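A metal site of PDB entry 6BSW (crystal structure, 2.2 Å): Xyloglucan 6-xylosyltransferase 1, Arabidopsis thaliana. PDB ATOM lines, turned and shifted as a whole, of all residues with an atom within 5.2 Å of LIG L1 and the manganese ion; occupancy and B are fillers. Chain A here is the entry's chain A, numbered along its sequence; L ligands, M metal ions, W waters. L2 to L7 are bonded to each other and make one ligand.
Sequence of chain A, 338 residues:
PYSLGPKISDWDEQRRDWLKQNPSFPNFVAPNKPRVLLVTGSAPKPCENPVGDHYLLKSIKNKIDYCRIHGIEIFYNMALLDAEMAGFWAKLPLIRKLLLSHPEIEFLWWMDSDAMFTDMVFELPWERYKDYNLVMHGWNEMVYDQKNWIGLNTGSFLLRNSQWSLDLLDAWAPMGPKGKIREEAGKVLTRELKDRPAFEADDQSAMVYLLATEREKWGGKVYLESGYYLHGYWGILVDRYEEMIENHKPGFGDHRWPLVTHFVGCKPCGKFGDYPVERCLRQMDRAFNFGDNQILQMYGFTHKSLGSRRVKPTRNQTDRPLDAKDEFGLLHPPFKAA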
ATOM      1  N   THR A  40      11.801 -29.327 -22.608  1.00  0.00           N
ATOM      2  CA  THR A  40      11.671 -27.943 -22.176  1.00  0.00           C
ATOM      3  C   THR A  40      12.639 -27.722 -21.017  1.00  0.00           C
ATOM      4  O   THR A  40      13.381 -28.625 -20.626  1.00  0.00           O
ATOM      5  CB  THR A  40      10.223 -27.617 -21.797  1.00  0.00           C
ATOM      6  OG1 THR A  40      10.116 -26.244 -21.423  1.00  0.00           O
ATOM      7  CG2 THR A  40       9.759 -28.494 -20.641  1.00  0.00           C
ATOM      8  N   GLY A  41      12.630 -26.514 -20.466  1.00  0.00           N
ATOM      9  CA  GLY A  41      13.521 -26.230 -19.356  1.00  0.00           C
ATOM     10  C   GLY A  41      13.399 -24.789 -18.907  1.00  0.00           C
ATOM     11  O   GLY A  41      12.755 -23.957 -19.563  1.00  0.00           O
ATOM     12  N   SER A  42      14.035 -24.511 -17.774  1.00  0.00           N
ATOM     13  CA  SER A  42      14.070 -23.175 -17.190  1.00  0.00           C
ATOM     14  C   SER A  42      15.271 -23.083 -16.269  1.00  0.00           C
ATOM     15  O   SER A  42      15.891 -24.089 -15.926  1.00  0.00           O
ATOM     16  CB  SER A  42      12.767 -22.865 -16.433  1.00  0.00           C
ATOM     17  OG  SER A  42      12.509 -23.838 -15.447  1.00  0.00           O
ATOM     18  N   ALA A  43      15.607 -21.852 -15.881  1.00  0.00           N
ATOM     19  CA  ALA A  43      16.794 -21.617 -15.085  1.00  0.00           C
ATOM     20  C   ALA A  43      16.664 -22.322 -13.728  1.00  0.00           C
ATOM     21  O   ALA A  43      15.564 -22.407 -13.166  1.00  0.00           O
ATOM     22  CB  ALA A  43      17.025 -20.122 -14.887  1.00  0.00           C
ATOM     23  N   GLY A  87      21.490 -18.824 -20.925  1.00  0.00           N
ATOM     24  CA  GLY A  87      20.273 -18.236 -21.439  1.00  0.00           C
ATOM     25  C   GLY A  87      19.547 -19.123 -22.427  1.00  0.00           C
ATOM     26  O   GLY A  87      19.505 -20.347 -22.262  1.00  0.00           O
ATOM     27  N   PHE A  88      18.976 -18.517 -23.468  1.00  0.00           N
ATOM     28  CA  PHE A  88      18.262 -19.284 -24.488  1.00  0.00           C
ATOM     29  C   PHE A  88      19.204 -20.119 -25.354  1.00  0.00           C
ATOM     30  O   PHE A  88      18.716 -20.951 -26.123  1.00  0.00           O
ATOM     31  CB  PHE A  88      17.410 -18.376 -25.385  1.00  0.00           C
ATOM     32  CG  PHE A  88      18.004 -17.029 -25.650  1.00  0.00           C
ATOM     33  CD1 PHE A  88      19.202 -16.899 -26.330  1.00  0.00           C
ATOM     34  CD2 PHE A  88      17.355 -15.880 -25.222  1.00  0.00           C
ATOM     35  CE1 PHE A  88      19.750 -15.650 -26.575  1.00  0.00           C
ATOM     36  CE2 PHE A  88      17.890 -14.631 -25.471  1.00  0.00           C
ATOM     37  CZ  PHE A  88      19.092 -14.519 -26.138  1.00  0.00           C
ATOM     38  N   ALA A  90      21.185 -22.264 -24.014  1.00  0.00           N
ATOM     39  CA  ALA A  90      21.439 -23.468 -23.229  1.00  0.00           C
ATOM     40  C   ALA A  90      20.817 -24.715 -23.851  1.00  0.00           C
ATOM     41  O   ALA A  90      21.181 -25.832 -23.470  1.00  0.00           O
ATOM     42  CB  ALA A  90      20.912 -23.297 -21.805  1.00  0.00           C
ATOM     43  N   LYS A  91      19.890 -24.556 -24.791  1.00  0.00           N
ATOM     44  CA  LYS A  91      19.213 -25.712 -25.363  1.00  0.00           C
ATOM     45  C   LYS A  91      20.050 -26.447 -26.393  1.00  0.00           C
ATOM     46  O   LYS A  91      19.764 -27.619 -26.680  1.00  0.00           O
ATOM     47  CB  LYS A  91      17.868 -25.310 -25.973  1.00  0.00           C
ATOM     48  CG  LYS A  91      17.926 -24.169 -26.976  1.00  0.00           C
ATOM     49  CD  LYS A  91      16.512 -23.712 -27.315  1.00  0.00           C
ATOM     50  CE  LYS A  91      16.522 -22.446 -28.165  1.00  0.00           C
ATOM     51  NZ  LYS A  91      15.154 -21.874 -28.318  1.00  0.00           N
ATOM     52  N   TRP A 110      11.656 -29.696 -29.004  1.00  0.00           N
ATOM     53  CA  TRP A 110      11.913 -28.639 -28.042  1.00  0.00           C
ATOM     54  C   TRP A 110      10.696 -27.722 -27.971  1.00  0.00           C
ATOM     55  O   TRP A 110      10.071 -27.405 -28.987  1.00  0.00           O
ATOM     56  CB  TRP A 110      13.140 -27.829 -28.421  1.00  0.00           C
ATOM     57  CG  TRP A 110      13.237 -26.573 -27.603  1.00  0.00           C
ATOM     58  CD1 TRP A 110      12.851 -25.318 -27.976  1.00  0.00           C
ATOM     59  CD2 TRP A 110      13.725 -26.461 -26.258  1.00  0.00           C
ATOM     60  NE1 TRP A 110      13.080 -24.431 -26.945  1.00  0.00           N
ATOM     61  CE2 TRP A 110      13.612 -25.111 -25.884  1.00  0.00           C
ATOM     62  CE3 TRP A 110      14.249 -27.385 -25.343  1.00  0.00           C
ATOM     63  CZ2 TRP A 110      14.002 -24.656 -24.631  1.00  0.00           C
ATOM     64  CZ3 TRP A 110      14.632 -26.924 -24.095  1.00  0.00           C
ATOM     65  CH2 TRP A 110      14.512 -25.572 -23.748  1.00  0.00           C
ATOM     66  N   MET A 111      10.376 -27.267 -26.751  1.00  0.00           N
ATOM     67  CA  MET A 111       9.262 -26.360 -26.546  1.00  0.00           C
ATOM     68  C   MET A 111       9.608 -25.398 -25.417  1.00  0.00           C
ATOM     69  O   MET A 111       9.934 -25.839 -24.308  1.00  0.00           O
ATOM     70  CB  MET A 111       7.973 -27.123 -26.214  1.00  0.00           C
ATOM     71  CG  MET A 111       6.730 -26.276 -26.301  1.00  0.00           C
ATOM     72  SD  MET A 111       5.228 -27.266 -26.331  1.00  0.00           S
ATOM     73  CE  MET A 111       3.983 -25.974 -26.396  1.00  0.00           C
ATOM     74  N   ASP A 112       9.528 -24.108 -25.707  1.00  0.00           N
ATOM     75  CA  ASP A 112       9.809 -23.074 -24.724  1.00  0.00           C
ATOM     76  C   ASP A 112       8.906 -23.213 -23.493  1.00  0.00           C
ATOM     77  O   ASP A 112       7.804 -23.758 -23.547  1.00  0.00           O
ATOM     78  CB  ASP A 112       9.609 -21.690 -25.335  1.00  0.00           C
ATOM     79  CG  ASP A 112      10.858 -21.147 -25.994  1.00  0.00           C
ATOM     80  OD1 ASP A 112      11.794 -21.933 -26.239  1.00  0.00           O
ATOM     81  OD2 ASP A 112      10.897 -19.927 -26.254  1.00  0.00           O
ATOM     82  N   SER A 113       9.402 -22.694 -22.366  1.00  0.00           N
ATOM     83  CA  SER A 113       8.615 -22.721 -21.143  1.00  0.00           C
ATOM     84  C   SER A 113       7.456 -21.727 -21.184  1.00  0.00           C
ATOM     85  O   SER A 113       6.444 -21.933 -20.500  1.00  0.00           O
ATOM     86  CB  SER A 113       9.499 -22.434 -19.928  1.00  0.00           C
ATOM     87  OG  SER A 113       9.991 -21.113 -19.956  1.00  0.00           O
ATOM     88  N   ASP A 114       7.581 -20.657 -21.967  1.00  0.00           N
ATOM     89  CA  ASP A 114       6.490 -19.704 -22.168  1.00  0.00           C
ATOM     90  C   ASP A 114       5.589 -20.100 -23.335  1.00  0.00           C
ATOM     91  O   ASP A 114       4.819 -19.266 -23.825  1.00  0.00           O
ATOM     92  CB  ASP A 114       7.034 -18.284 -22.372  1.00  0.00           C
ATOM     93  CG  ASP A 114       7.902 -18.152 -23.609  1.00  0.00           C
ATOM     94  OD1 ASP A 114       8.633 -19.108 -23.936  1.00  0.00           O
ATOM     95  OD2 ASP A 114       7.869 -17.081 -24.248  1.00  0.00           O
ATOM     96  N   HIS A 262       2.261 -19.023 -27.680  1.00  0.00           N
ATOM     97  CA  HIS A 262       3.624 -18.766 -27.229  1.00  0.00           C
ATOM     98  C   HIS A 262       3.727 -17.306 -26.832  1.00  0.00           C
ATOM     99  O   HIS A 262       3.504 -16.417 -27.660  1.00  0.00           O
ATOM    100  CB  HIS A 262       4.635 -19.130 -28.332  1.00  0.00           C
ATOM    101  CG  HIS A 262       6.061 -19.030 -27.901  1.00  0.00           C
ATOM    102  ND1 HIS A 262       7.114 -19.248 -28.777  1.00  0.00           N
ATOM    103  CD2 HIS A 262       6.620 -18.740 -26.702  1.00  0.00           C
ATOM    104  CE1 HIS A 262       8.251 -19.085 -28.134  1.00  0.00           C
ATOM    105  NE2 HIS A 262       7.991 -18.786 -26.875  1.00  0.00           N
ATOM    106  N   PHE A 263       4.080 -17.056 -25.575  1.00  0.00           N
ATOM    107  CA  PHE A 263       4.066 -15.703 -25.028  1.00  0.00           C
ATOM    108  C   PHE A 263       5.446 -15.049 -25.172  1.00  0.00           C
ATOM    109  O   PHE A 263       6.082 -14.611 -24.218  1.00  0.00           O
ATOM    110  CB  PHE A 263       3.590 -15.729 -23.579  1.00  0.00           C
ATOM    111  CG  PHE A 263       2.132 -16.028 -23.443  1.00  0.00           C
ATOM    112  CD1 PHE A 263       1.679 -17.334 -23.425  1.00  0.00           C
ATOM    113  CD2 PHE A 263       1.198 -15.006 -23.373  1.00  0.00           C
ATOM    114  CE1 PHE A 263       0.338 -17.623 -23.319  1.00  0.00           C
ATOM    115  CE2 PHE A 263      -0.148 -15.289 -23.273  1.00  0.00           C
ATOM    116  CZ  PHE A 263      -0.584 -16.596 -23.237  1.00  0.00           C
ATOM    117  N   VAL A 264       5.882 -14.977 -26.431  1.00  0.00           N
ATOM    118  CA  VAL A 264       7.147 -14.326 -26.764  1.00  0.00           C
ATOM    119  C   VAL A 264       7.129 -12.879 -26.299  1.00  0.00           C
ATOM    120  O   VAL A 264       6.126 -12.170 -26.436  1.00  0.00           O
ATOM    121  CB  VAL A 264       7.409 -14.424 -28.275  1.00  0.00           C
ATOM    122  CG1 VAL A 264       7.593 -15.869 -28.704  1.00  0.00           C
ATOM    123  CG2 VAL A 264       6.265 -13.769 -29.060  1.00  0.00           C
ATOM    124  N   GLY A 265       8.258 -12.431 -25.745  1.00  0.00           N
ATOM    125  CA  GLY A 265       8.407 -11.064 -25.314  1.00  0.00           C
ATOM    126  C   GLY A 265       7.870 -10.752 -23.929  1.00  0.00           C
ATOM    127  O   GLY A 265       8.063  -9.629 -23.460  1.00  0.00           O
ATOM    128  N   CYS A 266       7.232 -11.716 -23.268  1.00  0.00           N
ATOM    129  CA  CYS A 266       6.585 -11.455 -21.983  1.00  0.00           C
ATOM    130  C   CYS A 266       7.542 -11.607 -20.808  1.00  0.00           C
ATOM    131  O   CYS A 266       7.515 -10.786 -19.876  1.00  0.00           O
ATOM    132  CB  CYS A 266       5.385 -12.378 -21.816  1.00  0.00           C
ATOM    133  SG  CYS A 266       3.880 -11.756 -22.619  1.00  0.00           S
ATOM    134  N   LYS A 267       8.376 -12.635 -20.808  1.00  0.00           N
ATOM    135  CA  LYS A 267       9.323 -12.845 -19.723  1.00  0.00           C
ATOM    136  C   LYS A 267       8.597 -12.964 -18.390  1.00  0.00           C
ATOM    137  O   LYS A 267       8.861 -12.175 -17.470  1.00  0.00           O
ATOM    138  CB  LYS A 267      10.348 -11.707 -19.661  1.00  0.00           C
ATOM    139  CG  LYS A 267      11.068 -11.434 -20.967  1.00  0.00           C
ATOM    140  CD  LYS A 267      11.649 -12.714 -21.555  1.00  0.00           C
ATOM    141  CE  LYS A 267      12.415 -12.457 -22.838  1.00  0.00           C
ATOM    142  NZ  LYS A 267      12.587 -13.711 -23.624  1.00  0.00           N
HETATM  143  N1  LIG L   1      15.655 -21.170 -21.005  1.00  0.00           N
HETATM  144  C1  LIG L   1      16.492 -22.173 -20.309  1.00  0.00           C
HETATM  145  N2  LIG L   1      17.496 -21.713 -19.282  1.00  0.00           N
HETATM  146  C2  LIG L   1      17.654 -20.307 -18.968  1.00  0.00           C
HETATM  147  C3  LIG L   1      16.807 -19.297 -19.683  1.00  0.00           C
HETATM  148  C4  LIG L   1      15.821 -19.757 -20.693  1.00  0.00           C
HETATM  149  O1  LIG L   1      16.374 -23.310 -20.543  1.00  0.00           O
HETATM  150  O2  LIG L   1      18.458 -19.975 -18.154  1.00  0.00           O
HETATM  151  C5  LIG L   1      14.785 -21.585 -21.910  1.00  0.00           C
HETATM  152  C6  LIG L   1      13.327 -21.315 -21.488  1.00  0.00           C
HETATM  153  O3  LIG L   1      12.486 -22.442 -21.898  1.00  0.00           O
HETATM  154  C7  LIG L   1      12.987 -20.219 -22.162  1.00  0.00           C
HETATM  155  C8  LIG L   1      13.822 -20.308 -23.567  1.00  0.00           C
HETATM  156  O4  LIG L   1      15.001 -20.789 -23.248  1.00  0.00           O
HETATM  157  O5  LIG L   1      11.588 -20.190 -22.446  1.00  0.00           O
HETATM  158  C9  LIG L   1      13.955 -18.951 -24.157  1.00  0.00           C
HETATM  159  O6  LIG L   1      12.688 -18.532 -24.574  1.00  0.00           O
HETATM  160  P1  LIG L   1      12.104 -17.040 -24.162  1.00  0.00           P
HETATM  161  O7  LIG L   1      12.785 -16.482 -22.942  1.00  0.00           O
HETATM  162  O8  LIG L   1      10.617 -17.195 -23.892  1.00  0.00           O
HETATM  163  O9  LIG L   1      12.333 -16.006 -25.422  1.00  0.00           O
HETATM  164  P2  LIG L   1      11.054 -15.353 -26.223  1.00  0.00           P
HETATM  165  O10 LIG L   1      11.560 -14.529 -27.393  1.00  0.00           O
HETATM  166  O11 LIG L   1      10.200 -16.515 -26.712  1.00  0.00           O
HETATM  167  O12 LIG L   1      10.279 -14.470 -25.251  1.00  0.00           O
HETATM  168  C1  LG2 L   2      -0.698 -14.732 -42.093  1.00  0.00           C
HETATM  169  C2  LG2 L   2      -0.095 -13.614 -41.328  1.00  0.00           C
HETATM  170  C3  LG2 L   2       1.404 -13.601 -41.413  1.00  0.00           C
HETATM  171  C4  LG2 L   2       1.873 -13.629 -42.856  1.00  0.00           C
HETATM  172  C5  LG2 L   2       3.375 -13.705 -42.911  1.00  0.00           C
HETATM  173  C6  LG2 L   2      -0.188 -14.805 -43.521  1.00  0.00           C
HETATM  174  O1  LG2 L   2      -0.637 -15.947 -44.093  1.00  0.00           O
HETATM  175  O2  LG2 L   2      -2.142 -14.558 -42.128  1.00  0.00           O
HETATM  176  O3  LG2 L   2      -0.498 -13.741 -39.942  1.00  0.00           O
HETATM  177  O4  LG2 L   2       1.900 -12.404 -40.776  1.00  0.00           O
HETATM  178  O5  LG2 L   2       1.319 -14.794 -43.579  1.00  0.00           O
HETATM  179  O6  LG2 L   2       3.771 -14.033 -44.208  1.00  0.00           O
HETATM  180  C1  LG3 L   3       3.597 -11.404 -39.442  1.00  0.00           C
HETATM  181  C2  LG3 L   3       4.609 -11.631 -38.375  1.00  0.00           C
HETATM  182  C3  LG3 L   3       4.131 -12.463 -37.227  1.00  0.00           C
HETATM  183  C4  LG3 L   3       3.336 -13.700 -37.678  1.00  0.00           C
HETATM  184  C5  LG3 L   3       2.683 -14.360 -36.481  1.00  0.00           C
HETATM  185  C6  LG3 L   3       2.896 -12.696 -39.856  1.00  0.00           C
HETATM  186  O1  LG3 L   3       4.269 -10.862 -40.586  1.00  0.00           O
HETATM  187  O2  LG3 L   3       5.027 -10.337 -37.843  1.00  0.00           O
HETATM  188  O3  LG3 L   3       5.298 -12.908 -36.500  1.00  0.00           O
HETATM  189  O4  LG3 L   3       2.298 -13.376 -38.666  1.00  0.00           O
HETATM  190  O5  LG3 L   3       2.165 -15.626 -36.867  1.00  0.00           O
HETATM  191  C1  LG4 L   4       6.300 -13.419 -34.460  1.00  0.00           C
HETATM  192  C2  LG4 L   4       6.565 -12.996 -33.044  1.00  0.00           C
HETATM  193  C3  LG4 L   4       6.791 -11.529 -32.926  1.00  0.00           C
HETATM  194  C4  LG4 L   4       5.633 -10.755 -33.546  1.00  0.00           C
HETATM  195  C5  LG4 L   4       5.855  -9.266 -33.419  1.00  0.00           C
HETATM  196  C6  LG4 L   4       5.256 -12.579 -35.156  1.00  0.00           C
HETATM  197  O1  LG4 L   4       5.833 -14.777 -34.462  1.00  0.00           O
HETATM  198  O2  LG4 L   4       7.739 -13.699 -32.570  1.00  0.00           O
HETATM  199  O3  LG4 L   4       6.924 -11.167 -31.502  1.00  0.00           O
HETATM  200  O4  LG4 L   4       5.488 -11.105 -34.982  1.00  0.00           O
HETATM  201  O5  LG4 L   4       7.142  -8.935 -33.867  1.00  0.00           O
HETATM  202  C1  LG5 L   5       8.398 -10.366 -29.815  1.00  0.00           C
HETATM  203  C2  LG5 L   5       9.807 -10.261 -29.320  1.00  0.00           C
HETATM  204  C3  LG5 L   5      10.493 -11.566 -29.307  1.00  0.00           C
HETATM  205  C4  LG5 L   5      10.433 -12.227 -30.712  1.00  0.00           C
HETATM  206  C5  LG5 L   5      11.021 -13.509 -30.694  1.00  0.00           C
HETATM  207  C6  LG5 L   5       8.309 -11.006 -31.144  1.00  0.00           C
HETATM  208  O1  LG5 L   5       7.821  -9.015 -29.883  1.00  0.00           O
HETATM  209  O2  LG5 L   5       9.709  -9.663 -27.974  1.00  0.00           O
HETATM  210  O3  LG5 L   5      11.928 -11.504 -28.984  1.00  0.00           O
HETATM  211  O4  LG5 L   5       8.940 -12.325 -31.140  1.00  0.00           O
HETATM  212  O5  LG5 L   5      10.452 -14.304 -29.644  1.00  0.00           O
HETATM  213  C1  LG6 L   6      13.505 -11.246 -27.242  1.00  0.00           C
HETATM  214  C2  LG6 L   6      14.115 -10.345 -26.237  1.00  0.00           C
HETATM  215  C3  LG6 L   6      14.393  -8.980 -26.740  1.00  0.00           C
HETATM  216  C4  LG6 L   6      13.169  -8.329 -27.475  1.00  0.00           C
HETATM  217  C5  LG6 L   6      13.579  -7.150 -28.165  1.00  0.00           C
HETATM  218  C6  LG6 L   6      12.318 -10.655 -27.917  1.00  0.00           C
HETATM  219  O1  LG6 L   6      13.087 -12.461 -26.545  1.00  0.00           O
HETATM  220  O2  LG6 L   6      15.404 -10.957 -25.794  1.00  0.00           O
HETATM  221  O3  LG6 L   6      14.711  -8.146 -25.627  1.00  0.00           O
HETATM  222  O4  LG6 L   6      12.605  -9.336 -28.499  1.00  0.00           O
HETATM  223  O5  LG6 L   6      12.463  -6.625 -28.900  1.00  0.00           O
HETATM  224  C1  LG7 L   7      16.264  -6.627 -24.719  1.00  0.00           C
HETATM  225  C2  LG7 L   7      17.664  -6.405 -24.236  1.00  0.00           C
HETATM  226  C3  LG7 L   7      18.140  -7.546 -23.410  1.00  0.00           C
HETATM  227  C4  LG7 L   7      18.006  -8.864 -24.143  1.00  0.00           C
HETATM  228  C5  LG7 L   7      18.401  -9.978 -23.213  1.00  0.00           C
HETATM  229  C6  LG7 L   7      16.093  -7.956 -25.420  1.00  0.00           C
HETATM  230  O1  LG7 L   7      15.929  -5.580 -25.639  1.00  0.00           O
HETATM  231  O2  LG7 L   7      17.694  -5.198 -23.433  1.00  0.00           O
HETATM  232  O3  LG7 L   7      19.525  -7.330 -23.085  1.00  0.00           O
HETATM  233  O4  LG7 L   7      16.615  -9.096 -24.628  1.00  0.00           O
HETATM  234  O5  LG7 L   7      17.942 -11.201 -23.715  1.00  0.00           O
HETATM  235 MN    MN M   1       9.651 -18.296 -25.571  1.00  0.00          MN
HETATM  236  O   HOH W   1      10.544 -16.172 -21.264  1.00  0.00           O
HETATM  237  O   HOH W   2       8.854 -14.773 -23.044  1.00  0.00           O
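The side-chain hydroxyl (OG) of Ser 113 lies within hydrogen-bond range of an oxygen (O5) of LIG L1 (3.1 Å). An oxygen (O3) of LIG L1 is in hydrogen-bond range of the backbone carbonyl oxygen (O) of Gly 41 (2.8 Å). The side-chain amino group of Lys 267 lies within hydrogen-bond range of an oxygen (O1) of LG6 L6, 3.2 Å away. N of Ser 113 sits at hydrogen-bond distance from O3 of LIG L1, 3.1 Å away. N of Gly 265 is in hydrogen-bond range of O12 of LIG L1 (2.9 Å). An oxygen (O7) of LIG L1 lies within salt-bridge range of the side-chain amino group (NZ) of Lys 267, 2.9 Å away.
O10 of LIG L1 sits at hydrogen-bond distance from O5 of LG5 L5, at 2.5 Å.
OD1 of Asp 112 lies within salt-bridge range of NZ of Lys 91 (3.95 Å). The backbone carbonyl oxygen (O) of Asp 114 lies within hydrogen-bond range of the backbone NH (N) of Phe 263 (2.9 Å). The indole nitrogen of Trp 110 lies within hydrogen-bond range of the side-chain carboxylate of Asp 112 (2.9 Å).
Residues that only touch LIG L1: Ser 42, Ala 43, Gly 87, Phe 88, Trp 110 and Val 264. Hydrophobic or aromatic side chains within 4 Å of LIG L1: Ala 43, Phe 88, Trp 110, His 262 and Val 264. 13 residues have an atom within 4 Å of LIG L1: Gly 41, Ser 42, Ala 43, Gly 87, Phe 88, Trp 110, Asp 112, Ser 113, Asp 114, His 262, Val 264, Gly 265 and Lys 267. Along chain A the residues within 4 Å of LIG L1 span positions 41 to 267.
Three residues have an atom within 4 Å of the manganese ion: Asp 112, Asp 114 and His 262.
The manganese ion is bound by OD1 of Asp 114, OD2 of Asp 112, NE2 of His 262, O11 of LIG L1, O8 of LIG L1 and OD2 of Asp 114. The manganese ion has six donor atoms within binding distance.
Water W2 lies within hydrogen-bond range of O12 of LIG L1, O of Phe 263, N of Lys 267 and N of Cys 266.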
